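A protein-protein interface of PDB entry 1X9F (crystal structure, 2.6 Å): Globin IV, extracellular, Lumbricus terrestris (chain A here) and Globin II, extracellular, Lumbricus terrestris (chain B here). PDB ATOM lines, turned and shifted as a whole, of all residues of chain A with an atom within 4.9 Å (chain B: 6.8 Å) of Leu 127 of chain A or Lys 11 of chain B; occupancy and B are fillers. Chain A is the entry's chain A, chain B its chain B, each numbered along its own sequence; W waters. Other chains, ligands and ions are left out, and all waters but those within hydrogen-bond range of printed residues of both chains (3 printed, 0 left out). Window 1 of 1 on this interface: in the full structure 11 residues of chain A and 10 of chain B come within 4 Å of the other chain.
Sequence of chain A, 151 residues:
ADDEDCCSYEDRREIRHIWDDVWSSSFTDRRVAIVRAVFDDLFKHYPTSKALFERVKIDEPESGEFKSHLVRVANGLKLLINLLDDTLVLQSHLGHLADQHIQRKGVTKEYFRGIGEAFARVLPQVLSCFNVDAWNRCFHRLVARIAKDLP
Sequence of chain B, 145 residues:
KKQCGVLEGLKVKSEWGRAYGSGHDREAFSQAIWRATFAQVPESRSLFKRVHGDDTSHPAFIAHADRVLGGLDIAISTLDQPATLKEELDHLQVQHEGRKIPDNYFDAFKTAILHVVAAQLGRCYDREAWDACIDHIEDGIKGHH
OE2 of Glu 15 of chain B sits at hydrogen-bond distance from NE1 of Trp 130 of chain B (2.8 Å). NZ of Lys 11 of chain B is in salt-bridge range of OD2 of Asp 126 of chain B. The side-chain carboxylate of Asp 126 of chain B is in hydrogen-bond range of the backbone NH of Ala 129 of chain B. NZ of Lys 2 of chain B lies within salt-bridge range of OD2 of Asp 126 of chain B, at 3.1 Å. The backbone NH (N) of Asp 126 of chain B lies within hydrogen-bond range of the side-chain carboxylate (OE2) of Glu 15 of chain B, at 3.2 Å.
Of the printed residues of chain B, Pro 124 of chain A touches Lys 11 (3.0 Å). Printed residues of chain B within 4 Å of Leu 127 of chain A: Lys 11. Of chain A, only Pro 124, Gln 125, Val 126, Leu 127 and Ser 128 come within 4 Å of Lys 11 of chain B. Trp 16 of chain B touches none of the printed residues of chain A. Printed residues of chain A within 4 Å of Arg 18 of chain B: Asp 21. Printed residues of chain A within 4 Å of Tyr 125 of chain B: Ser 128 (3.6 Å). Printed residues of chain A within 4 Å of Asp 126 of chain B: Ser 128 (3.7 Å). The nearest residue of chain B that does not touch Leu 127 of chain A is Glu 15 of chain B (5.0 Å). The nearest printed residue of chain A that does not touch Lys 11 of chain B is Leu 123 of chain A (5.6 Å).
Water W3 lies within hydrogen-bond range of OD2 of Asp 126 of chain B (2.4 Å), NZ of Lys 11 of chain B (2.8 Å) and O of Gln 125 of chain A (3.3 Å). Water W1 lies within hydrogen-bond range of the backbone NH (N) of Ser 128 of chain A (2.6 Å), the side-chain carboxylate (OE1) of Glu 15 of chain B (2.8 Å) and the guanidinium group (NH2) of Arg 18 of chain B (3.0 Å). Water W2 lies within hydrogen-bond range of the side-chain hydroxyl (OG) of Ser 14 of chain B (2.7 Å) and the backbone carbonyl oxygen (O) of Asp 21 of chain A (2.7 Å).
Among the printed residues, merely in contact across the chains: Gln 125 of chain A with Lys 11 of chain B (3.3 Å), Ser 128 of chain A with Tyr 125 of chain B (3.6 Å), Leu 127 of chain A with Lys 11 of chain B (3.6 Å), Val 126 of chain A with Lys 11 of chain B (3.6 Å) and Ser 128 of chain A with Asp 126 of chain B (3.7 Å).
O of Leu 7 of chain B lies close to O of Gln 125 of chain A, 3.5 Å away. OG of Ser 128 of chain A lies within hydrogen-bond range of NZ of Lys 11 of chain B. The side-chain carboxylate (OD2) of Asp 21 of chain A is in salt-bridge range of the guanidinium group (NH1) of Arg 18 of chain B (2.8 Å). The side-chain hydroxyl (OG) of Ser 128 of chain A lies within hydrogen-bond range of the side-chain carboxylate (OE1) of Glu 15 of chain B, at 2.7 Å. NZ of Lys 11 of chain B sits at hydrogen-bond distance from O of Pro 124 of chain A, 3.0 Å away.
Of the 11 printed residues of chain A, 6 touch a printed residue of chain B. Along chain A the printed residues that touch a printed residue of chain B span positions 21 to 128. Of the 20 printed residues of chain B, 6 touch a printed residue of chain A. Among the printed residues, Asp or Glu carboxylates within 4 Å of a Lys or Arg side-chain nitrogen of the other chain: Asp 21 of chain A with Arg 18 of chain B (2.8 Å).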
ATOM      1  N   ILE A  18      35.701  10.040  -0.932  1.00  0.00           N
ATOM      2  CA  ILE A  18      35.090  10.533  -2.167  1.00  0.00           C
ATOM      3  C   ILE A  18      36.129  10.554  -3.284  1.00  0.00           C
ATOM      4  O   ILE A  18      35.898  10.024  -4.373  1.00  0.00           O
ATOM      5  CB  ILE A  18      34.494  11.961  -1.962  1.00  0.00           C
ATOM      6  CG1 ILE A  18      33.148  11.911  -1.214  1.00  0.00           C
ATOM      7  CG2 ILE A  18      34.372  12.716  -3.296  1.00  0.00           C
ATOM      8  CD1 ILE A  18      32.156  10.853  -1.708  1.00  0.00           C
ATOM      9  N   ASP A  21      37.355   7.803  -5.641  1.00  0.00           N
ATOM     10  CA  ASP A  21      36.437   7.352  -6.689  1.00  0.00           C
ATOM     11  C   ASP A  21      36.413   8.220  -7.948  1.00  0.00           C
ATOM     12  O   ASP A  21      36.273   7.682  -9.048  1.00  0.00           O
ATOM     13  CB  ASP A  21      35.013   7.184  -6.141  1.00  0.00           C
ATOM     14  CG  ASP A  21      34.849   5.917  -5.310  1.00  0.00           C
ATOM     15  OD1 ASP A  21      35.735   5.619  -4.478  1.00  0.00           O
ATOM     16  OD2 ASP A  21      33.857   5.162  -5.410  1.00  0.00           O
ATOM     17  N   VAL A  22      36.527   9.544  -7.801  1.00  0.00           N
ATOM     18  CA  VAL A  22      36.612  10.443  -8.969  1.00  0.00           C
ATOM     19  C   VAL A  22      37.977  10.313  -9.659  1.00  0.00           C
ATOM     20  O   VAL A  22      38.064  10.179 -10.885  1.00  0.00           O
ATOM     21  CB  VAL A  22      36.369  11.942  -8.605  1.00  0.00           C
ATOM     22  CG1 VAL A  22      34.956  12.166  -8.082  1.00  0.00           C
ATOM     23  CG2 VAL A  22      37.378  12.414  -7.589  1.00  0.00           C
ATOM     24  N   LEU A 123      29.979  16.757  -9.610  1.00  0.00           N
ATOM     25  CA  LEU A 123      30.438  15.596  -8.830  1.00  0.00           C
ATOM     26  C   LEU A 123      29.323  14.589  -8.519  1.00  0.00           C
ATOM     27  O   LEU A 123      29.498  13.392  -8.767  1.00  0.00           O
ATOM     28  CB  LEU A 123      31.191  16.015  -7.561  1.00  0.00           C
ATOM     29  CG  LEU A 123      32.587  16.602  -7.793  1.00  0.00           C
ATOM     30  CD1 LEU A 123      33.258  16.898  -6.471  1.00  0.00           C
ATOM     31  CD2 LEU A 123      33.458  15.666  -8.623  1.00  0.00           C
ATOM     32  N   PRO A 124      28.174  15.050  -8.017  1.00  0.00           N
ATOM     33  CA  PRO A 124      27.051  14.140  -7.736  1.00  0.00           C
ATOM     34  C   PRO A 124      26.569  13.351  -8.960  1.00  0.00           C
ATOM     35  O   PRO A 124      25.873  12.346  -8.801  1.00  0.00           O
ATOM     36  CB  PRO A 124      25.945  15.071  -7.220  1.00  0.00           C
ATOM     37  CG  PRO A 124      26.341  16.436  -7.634  1.00  0.00           C
ATOM     38  CD  PRO A 124      27.847  16.448  -7.672  1.00  0.00           C
ATOM     39  N   GLN A 125      26.943  13.796 -10.158  1.00  0.00           N
ATOM     40  CA  GLN A 125      26.613  13.075 -11.389  1.00  0.00           C
ATOM     41  C   GLN A 125      27.653  12.021 -11.764  1.00  0.00           C
ATOM     42  O   GLN A 125      27.354  11.118 -12.546  1.00  0.00           O
ATOM     43  CB  GLN A 125      26.433  14.039 -12.563  1.00  0.00           C
ATOM     44  CG  GLN A 125      25.100  14.755 -12.621  1.00  0.00           C
ATOM     45  CD  GLN A 125      25.099  15.839 -13.677  1.00  0.00           C
ATOM     46  OE1 GLN A 125      25.354  17.005 -13.375  1.00  0.00           O
ATOM     47  NE2 GLN A 125      24.852  15.463 -14.928  1.00  0.00           N
ATOM     48  N   VAL A 126      28.867  12.133 -11.234  1.00  0.00           N
ATOM     49  CA  VAL A 126      29.897  11.150 -11.566  1.00  0.00           C
ATOM     50  C   VAL A 126      30.038  10.079 -10.490  1.00  0.00           C
ATOM     51  O   VAL A 126      30.502   8.972 -10.773  1.00  0.00           O
ATOM     52  CB  VAL A 126      31.273  11.787 -11.910  1.00  0.00           C
ATOM     53  CG1 VAL A 126      31.101  12.930 -12.913  1.00  0.00           C
ATOM     54  CG2 VAL A 126      32.001  12.265 -10.661  1.00  0.00           C
ATOM     55  N   LEU A 127      29.640  10.395  -9.262  1.00  0.00           N
ATOM     56  CA  LEU A 127      29.628   9.369  -8.232  1.00  0.00           C
ATOM     57  C   LEU A 127      28.422   9.460  -7.302  1.00  0.00           C
ATOM     58  O   LEU A 127      27.923  10.551  -7.012  1.00  0.00           O
ATOM     59  CB  LEU A 127      30.963   9.315  -7.466  1.00  0.00           C
ATOM     60  CG  LEU A 127      31.309  10.330  -6.377  1.00  0.00           C
ATOM     61  CD1 LEU A 127      32.470   9.826  -5.532  1.00  0.00           C
ATOM     62  CD2 LEU A 127      31.618  11.703  -6.942  1.00  0.00           C
ATOM     63  N   SER A 128      27.947   8.303  -6.857  1.00  0.00           N
ATOM     64  CA  SER A 128      26.813   8.238  -5.940  1.00  0.00           C
ATOM     65  C   SER A 128      27.312   8.153  -4.495  1.00  0.00           C
ATOM     66  O   SER A 128      28.507   7.936  -4.258  1.00  0.00           O
ATOM     67  CB  SER A 128      25.912   7.044  -6.282  1.00  0.00           C
ATOM     68  OG  SER A 128      25.557   7.059  -7.664  1.00  0.00           O
ATOM     69  N   CYS A 129      26.396   8.324  -3.538  1.00  0.00           N
ATOM     70  CA  CYS A 129      26.749   8.415  -2.115  1.00  0.00           C
ATOM     71  C   CYS A 129      27.821   9.486  -1.906  1.00  0.00           C
ATOM     72  O   CYS A 129      28.747   9.324  -1.104  1.00  0.00           O
ATOM     73  CB  CYS A 129      27.221   7.066  -1.552  1.00  0.00           C
ATOM     74  SG  CYS A 129      26.037   5.701  -1.646  1.00  0.00           S
ATOM     75  N   PHE A 130      27.681  10.580  -2.644  1.00  0.00           N
ATOM     76  CA  PHE A 130      28.612  11.682  -2.555  1.00  0.00           C
ATOM     77  C   PHE A 130      28.096  12.669  -1.522  1.00  0.00           C
ATOM     78  O   PHE A 130      26.972  13.154  -1.639  1.00  0.00           O
ATOM     79  CB  PHE A 130      28.743  12.342  -3.927  1.00  0.00           C
ATOM     80  CG  PHE A 130      29.561  13.592  -3.929  1.00  0.00           C
ATOM     81  CD1 PHE A 130      30.911  13.561  -3.612  1.00  0.00           C
ATOM     82  CD2 PHE A 130      28.988  14.803  -4.282  1.00  0.00           C
ATOM     83  CE1 PHE A 130      31.670  14.723  -3.626  1.00  0.00           C
ATOM     84  CE2 PHE A 130      29.741  15.968  -4.300  1.00  0.00           C
ATOM     85  CZ  PHE A 130      31.084  15.925  -3.971  1.00  0.00           C
ATOM     86  N   LYS B   2      16.555  10.529 -18.691  1.00  0.00           N
ATOM     87  CA  LYS B   2      17.954  10.945 -18.687  1.00  0.00           C
ATOM     88  C   LYS B   2      18.622  10.218 -19.855  1.00  0.00           C
ATOM     89  O   LYS B   2      18.266   9.080 -20.159  1.00  0.00           O
ATOM     90  CB  LYS B   2      18.609  10.556 -17.360  1.00  0.00           C
ATOM     91  CG  LYS B   2      20.005  11.103 -17.145  1.00  0.00           C
ATOM     92  CD  LYS B   2      20.579  10.621 -15.822  1.00  0.00           C
ATOM     93  CE  LYS B   2      20.223  11.577 -14.669  1.00  0.00           C
ATOM     94  NZ  LYS B   2      20.744  11.024 -13.359  1.00  0.00           N
ATOM     95  N   GLY B   5      24.680  10.304 -21.463  1.00  0.00           N
ATOM     96  CA  GLY B   5      25.687  11.297 -21.782  1.00  0.00           C
ATOM     97  C   GLY B   5      27.023  10.998 -21.131  1.00  0.00           C
ATOM     98  O   GLY B   5      27.227   9.933 -20.536  1.00  0.00           O
ATOM     99  N   VAL B   6      27.926  11.964 -21.255  1.00  0.00           N
ATOM    100  CA  VAL B   6      29.287  11.849 -20.750  1.00  0.00           C
ATOM    101  C   VAL B   6      29.303  11.464 -19.270  1.00  0.00           C
ATOM    102  O   VAL B   6      29.967  10.503 -18.883  1.00  0.00           O
ATOM    103  CB  VAL B   6      30.080  13.169 -20.986  1.00  0.00           C
ATOM    104  CG1 VAL B   6      31.421  13.156 -20.253  1.00  0.00           C
ATOM    105  CG2 VAL B   6      30.281  13.420 -22.484  1.00  0.00           C
ATOM    106  N   LEU B   7      28.557  12.205 -18.455  1.00  0.00           N
ATOM    107  CA  LEU B   7      28.584  12.034 -17.004  1.00  0.00           C
ATOM    108  C   LEU B   7      27.949  10.726 -16.538  1.00  0.00           C
ATOM    109  O   LEU B   7      28.494  10.045 -15.665  1.00  0.00           O
ATOM    110  CB  LEU B   7      27.931  13.238 -16.315  1.00  0.00           C
ATOM    111  CG  LEU B   7      28.794  14.437 -15.874  1.00  0.00           C
ATOM    112  CD1 LEU B   7      30.100  14.599 -16.670  1.00  0.00           C
ATOM    113  CD2 LEU B   7      27.983  15.744 -15.895  1.00  0.00           C
ATOM    114  N   GLU B   8      26.801  10.381 -17.120  1.00  0.00           N
ATOM    115  CA  GLU B   8      26.127   9.109 -16.829  1.00  0.00           C
ATOM    116  C   GLU B   8      26.962   7.908 -17.267  1.00  0.00           C
ATOM    117  O   GLU B   8      26.990   6.888 -16.583  1.00  0.00           O
ATOM    118  CB  GLU B   8      24.712   9.060 -17.429  1.00  0.00           C
ATOM    119  CG  GLU B   8      24.434  10.051 -18.553  1.00  0.00           C
ATOM    120  CD  GLU B   8      24.197  11.478 -18.076  1.00  0.00           C
ATOM    121  OE1 GLU B   8      23.262  11.707 -17.278  1.00  0.00           O
ATOM    122  OE2 GLU B   8      24.947  12.379 -18.513  1.00  0.00           O
ATOM    123  N   GLY B   9      27.650   8.044 -18.398  1.00  0.00           N
ATOM    124  CA  GLY B   9      28.560   7.009 -18.880  1.00  0.00           C
ATOM    125  C   GLY B   9      29.734   6.846 -17.935  1.00  0.00           C
ATOM    126  O   GLY B   9      30.149   5.722 -17.632  1.00  0.00           O
ATOM    127  N   LEU B  10      30.264   7.973 -17.470  1.00  0.00           N
ATOM    128  CA  LEU B  10      31.312   7.960 -16.461  1.00  0.00           C
ATOM    129  C   LEU B  10      30.850   7.206 -15.220  1.00  0.00           C
ATOM    130  O   LEU B  10      31.547   6.309 -14.752  1.00  0.00           O
ATOM    131  CB  LEU B  10      31.741   9.388 -16.101  1.00  0.00           C
ATOM    132  CG  LEU B  10      33.117   9.929 -16.518  1.00  0.00           C
ATOM    133  CD1 LEU B  10      33.750   9.197 -17.707  1.00  0.00           C
ATOM    134  CD2 LEU B  10      33.047  11.432 -16.776  1.00  0.00           C
ATOM    135  N   LYS B  11      29.673   7.557 -14.705  1.00  0.00           N
ATOM    136  CA  LYS B  11      29.144   6.945 -13.485  1.00  0.00           C
ATOM    137  C   LYS B  11      28.900   5.443 -13.649  1.00  0.00           C
ATOM    138  O   LYS B  11      29.296   4.642 -12.794  1.00  0.00           O
ATOM    139  CB  LYS B  11      27.863   7.650 -13.036  1.00  0.00           C
ATOM    140  CG  LYS B  11      27.287   7.068 -11.759  1.00  0.00           C
ATOM    141  CD  LYS B  11      26.101   7.856 -11.270  1.00  0.00           C
ATOM    142  CE  LYS B  11      26.518   8.907 -10.270  1.00  0.00           C
ATOM    143  NZ  LYS B  11      25.320   9.553  -9.678  1.00  0.00           N
ATOM    144  N   VAL B  12      28.256   5.077 -14.755  1.00  0.00           N
ATOM    145  CA  VAL B  12      27.971   3.676 -15.046  1.00  0.00           C
ATOM    146  C   VAL B  12      29.247   2.851 -15.211  1.00  0.00           C
ATOM    147  O   VAL B  12      29.291   1.708 -14.751  1.00  0.00           O
ATOM    148  CB  VAL B  12      27.027   3.500 -16.257  1.00  0.00           C
ATOM    149  CG1 VAL B  12      26.865   2.024 -16.611  1.00  0.00           C
ATOM    150  CG2 VAL B  12      25.664   4.116 -15.964  1.00  0.00           C
ATOM    151  N   LYS B  13      30.280   3.416 -15.846  1.00  0.00           N
ATOM    152  CA  LYS B  13      31.568   2.710 -15.937  1.00  0.00           C
ATOM    153  C   LYS B  13      32.091   2.331 -14.551  1.00  0.00           C
ATOM    154  O   LYS B  13      32.473   1.181 -14.323  1.00  0.00           O
ATOM    155  CB  LYS B  13      32.613   3.525 -16.712  1.00  0.00           C
ATOM    156  CG  LYS B  13      32.376   3.507 -18.228  1.00  0.00           C
ATOM    157  CD  LYS B  13      33.463   4.306 -18.974  1.00  0.00           C
ATOM    158  CE  LYS B  13      34.834   3.608 -18.863  1.00  0.00           C
ATOM    159  NZ  LYS B  13      35.861   4.358 -19.659  1.00  0.00           N
ATOM    160  N   SER B  14      32.082   3.285 -13.624  1.00  0.00           N
ATOM    161  CA  SER B  14      32.580   3.042 -12.267  1.00  0.00           C
ATOM    162  C   SER B  14      31.731   2.058 -11.481  1.00  0.00           C
ATOM    163  O   SER B  14      32.260   1.137 -10.849  1.00  0.00           O
ATOM    164  CB  SER B  14      32.685   4.347 -11.482  1.00  0.00           C
ATOM    165  OG  SER B  14      33.825   5.079 -11.890  1.00  0.00           O
ATOM    166  N   GLU B  15      30.417   2.267 -11.505  1.00  0.00           N
ATOM    167  CA  GLU B  15      29.513   1.412 -10.763  1.00  0.00           C
ATOM    168  C   GLU B  15      29.518  -0.004 -11.320  1.00  0.00           C
ATOM    169  O   GLU B  15      29.365  -0.966 -10.566  1.00  0.00           O
ATOM    170  CB  GLU B  15      28.122   2.038 -10.704  1.00  0.00           C
ATOM    171  CG  GLU B  15      28.178   3.364  -9.954  1.00  0.00           C
ATOM    172  CD  GLU B  15      26.848   4.069  -9.834  1.00  0.00           C
ATOM    173  OE1 GLU B  15      26.782   5.047  -9.057  1.00  0.00           O
ATOM    174  OE2 GLU B  15      25.875   3.660 -10.506  1.00  0.00           O
ATOM    175  N   TRP B  16      29.736  -0.137 -12.628  1.00  0.00           N
ATOM    176  CA  TRP B  16      29.881  -1.456 -13.242  1.00  0.00           C
ATOM    177  C   TRP B  16      31.123  -2.156 -12.701  1.00  0.00           C
ATOM    178  O   TRP B  16      31.051  -3.302 -12.254  1.00  0.00           O
ATOM    179  CB  TRP B  16      29.931  -1.361 -14.773  1.00  0.00           C
ATOM    180  CG  TRP B  16      30.329  -2.645 -15.438  1.00  0.00           C
ATOM    181  CD1 TRP B  16      31.543  -2.935 -15.999  1.00  0.00           C
ATOM    182  CD2 TRP B  16      29.526  -3.825 -15.590  1.00  0.00           C
ATOM    183  NE1 TRP B  16      31.544  -4.217 -16.496  1.00  0.00           N
ATOM    184  CE2 TRP B  16      30.320  -4.787 -16.261  1.00  0.00           C
ATOM    185  CE3 TRP B  16      28.211  -4.170 -15.235  1.00  0.00           C
ATOM    186  CZ2 TRP B  16      29.844  -6.059 -16.587  1.00  0.00           C
ATOM    187  CZ3 TRP B  16      27.738  -5.438 -15.561  1.00  0.00           C
ATOM    188  CH2 TRP B  16      28.554  -6.365 -16.230  1.00  0.00           C
ATOM    189  N   GLY B  17      32.252  -1.449 -12.740  1.00  0.00           N
ATOM    190  CA  GLY B  17      33.506  -1.941 -12.178  1.00  0.00           C
ATOM    191  C   GLY B  17      33.330  -2.498 -10.779  1.00  0.00           C
ATOM    192  O   GLY B  17      33.727  -3.633 -10.506  1.00  0.00           O
ATOM    193  N   ARG B  18      32.717  -1.712  -9.899  1.00  0.00           N
ATOM    194  CA  ARG B  18      32.475  -2.147  -8.527  1.00  0.00           C
ATOM    195  C   ARG B  18      31.519  -3.339  -8.383  1.00  0.00           C
ATOM    196  O   ARG B  18      31.687  -4.145  -7.470  1.00  0.00           O
ATOM    197  CB  ARG B  18      31.990  -0.978  -7.676  1.00  0.00           C
ATOM    198  CG  ARG B  18      33.041  -0.440  -6.724  1.00  0.00           C
ATOM    199  CD  ARG B  18      33.290   1.048  -6.874  1.00  0.00           C
ATOM    200  NE  ARG B  18      32.050   1.819  -6.869  1.00  0.00           N
ATOM    201  CZ  ARG B  18      31.944   3.082  -7.270  1.00  0.00           C
ATOM    202  NH1 ARG B  18      33.007   3.744  -7.719  1.00  0.00           N
ATOM    203  NH2 ARG B  18      30.766   3.688  -7.224  1.00  0.00           N
ATOM    204  N   TYR B 125      24.299   3.798  -6.253  1.00  0.00           N
ATOM    205  CA  TYR B 125      24.141   3.630  -7.677  1.00  0.00           C
ATOM    206  C   TYR B 125      23.064   4.576  -8.176  1.00  0.00           C
ATOM    207  O   TYR B 125      22.216   5.027  -7.403  1.00  0.00           O
ATOM    208  CB  TYR B 125      23.884   2.154  -8.026  1.00  0.00           C
ATOM    209  CG  TYR B 125      22.481   1.812  -8.439  1.00  0.00           C
ATOM    210  CD1 TYR B 125      21.403   2.031  -7.587  1.00  0.00           C
ATOM    211  CD2 TYR B 125      22.239   1.243  -9.679  1.00  0.00           C
ATOM    212  CE1 TYR B 125      20.120   1.720  -7.970  1.00  0.00           C
ATOM    213  CE2 TYR B 125      20.964   0.921 -10.072  1.00  0.00           C
ATOM    214  CZ  TYR B 125      19.909   1.164  -9.214  1.00  0.00           C
ATOM    215  OH  TYR B 125      18.635   0.836  -9.600  1.00  0.00           O
ATOM    216  N   ASP B 126      23.123   4.896  -9.462  1.00  0.00           N
ATOM    217  CA  ASP B 126      22.163   5.797 -10.071  1.00  0.00           C
ATOM    218  C   ASP B 126      21.362   5.062 -11.139  1.00  0.00           C
ATOM    219  O   ASP B 126      21.837   4.834 -12.259  1.00  0.00           O
ATOM    220  CB  ASP B 126      22.893   7.001 -10.656  1.00  0.00           C
ATOM    221  CG  ASP B 126      21.955   8.019 -11.278  1.00  0.00           C
ATOM    222  OD1 ASP B 126      20.856   7.655 -11.749  1.00  0.00           O
ATOM    223  OD2 ASP B 126      22.253   9.228 -11.353  1.00  0.00           O
ATOM    224  N   ARG B 127      20.137   4.712 -10.767  1.00  0.00           N
ATOM    225  CA  ARG B 127      19.224   3.937 -11.590  1.00  0.00           C
ATOM    226  C   ARG B 127      18.922   4.615 -12.923  1.00  0.00           C
ATOM    227  O   ARG B 127      18.872   3.956 -13.966  1.00  0.00           O
ATOM    228  CB  ARG B 127      17.931   3.719 -10.810  1.00  0.00           C
ATOM    229  CG  ARG B 127      16.911   2.897 -11.531  1.00  0.00           C
ATOM    230  CD  ARG B 127      15.723   2.496 -10.693  1.00  0.00           C
ATOM    231  NE  ARG B 127      15.092   1.331 -11.300  1.00  0.00           N
ATOM    232  CZ  ARG B 127      14.272   1.370 -12.345  1.00  0.00           C
ATOM    233  NH1 ARG B 127      13.941   2.527 -12.912  1.00  0.00           N
ATOM    234  NH2 ARG B 127      13.766   0.240 -12.822  1.00  0.00           N
ATOM    235  N   ALA B 129      20.793   6.768 -14.556  1.00  0.00           N
ATOM    236  CA  ALA B 129      21.994   6.744 -15.387  1.00  0.00           C
ATOM    237  C   ALA B 129      22.215   5.352 -15.979  1.00  0.00           C
ATOM    238  O   ALA B 129      22.558   5.225 -17.162  1.00  0.00           O
ATOM    239  CB  ALA B 129      23.211   7.191 -14.582  1.00  0.00           C
ATOM    240  N   TRP B 130      22.008   4.312 -15.173  1.00  0.00           N
ATOM    241  CA  TRP B 130      22.096   2.937 -15.663  1.00  0.00           C
ATOM    242  C   TRP B 130      21.031   2.643 -16.709  1.00  0.00           C
ATOM    243  O   TRP B 130      21.341   2.137 -17.787  1.00  0.00           O
ATOM    244  CB  TRP B 130      21.991   1.934 -14.516  1.00  0.00           C
ATOM    245  CG  TRP B 130      23.283   1.669 -13.835  1.00  0.00           C
ATOM    246  CD1 TRP B 130      23.847   2.409 -12.836  1.00  0.00           C
ATOM    247  CD2 TRP B 130      24.185   0.587 -14.092  1.00  0.00           C
ATOM    248  NE1 TRP B 130      25.045   1.855 -12.453  1.00  0.00           N
ATOM    249  CE2 TRP B 130      25.277   0.733 -13.204  1.00  0.00           C
ATOM    250  CE3 TRP B 130      24.182  -0.500 -14.979  1.00  0.00           C
ATOM    251  CZ2 TRP B 130      26.355  -0.162 -13.179  1.00  0.00           C
ATOM    252  CZ3 TRP B 130      25.250  -1.388 -14.952  1.00  0.00           C
ATOM    253  CH2 TRP B 130      26.322  -1.212 -14.057  1.00  0.00           C
HETATM  254  O   HOH W   1      29.043   6.118  -7.811  1.00  0.00           O
HETATM  255  O   HOH W   2      35.864   5.241 -10.134  1.00  0.00           O
HETATM  256  O   HOH W   3      24.096  10.673 -11.909  1.00  0.00           O
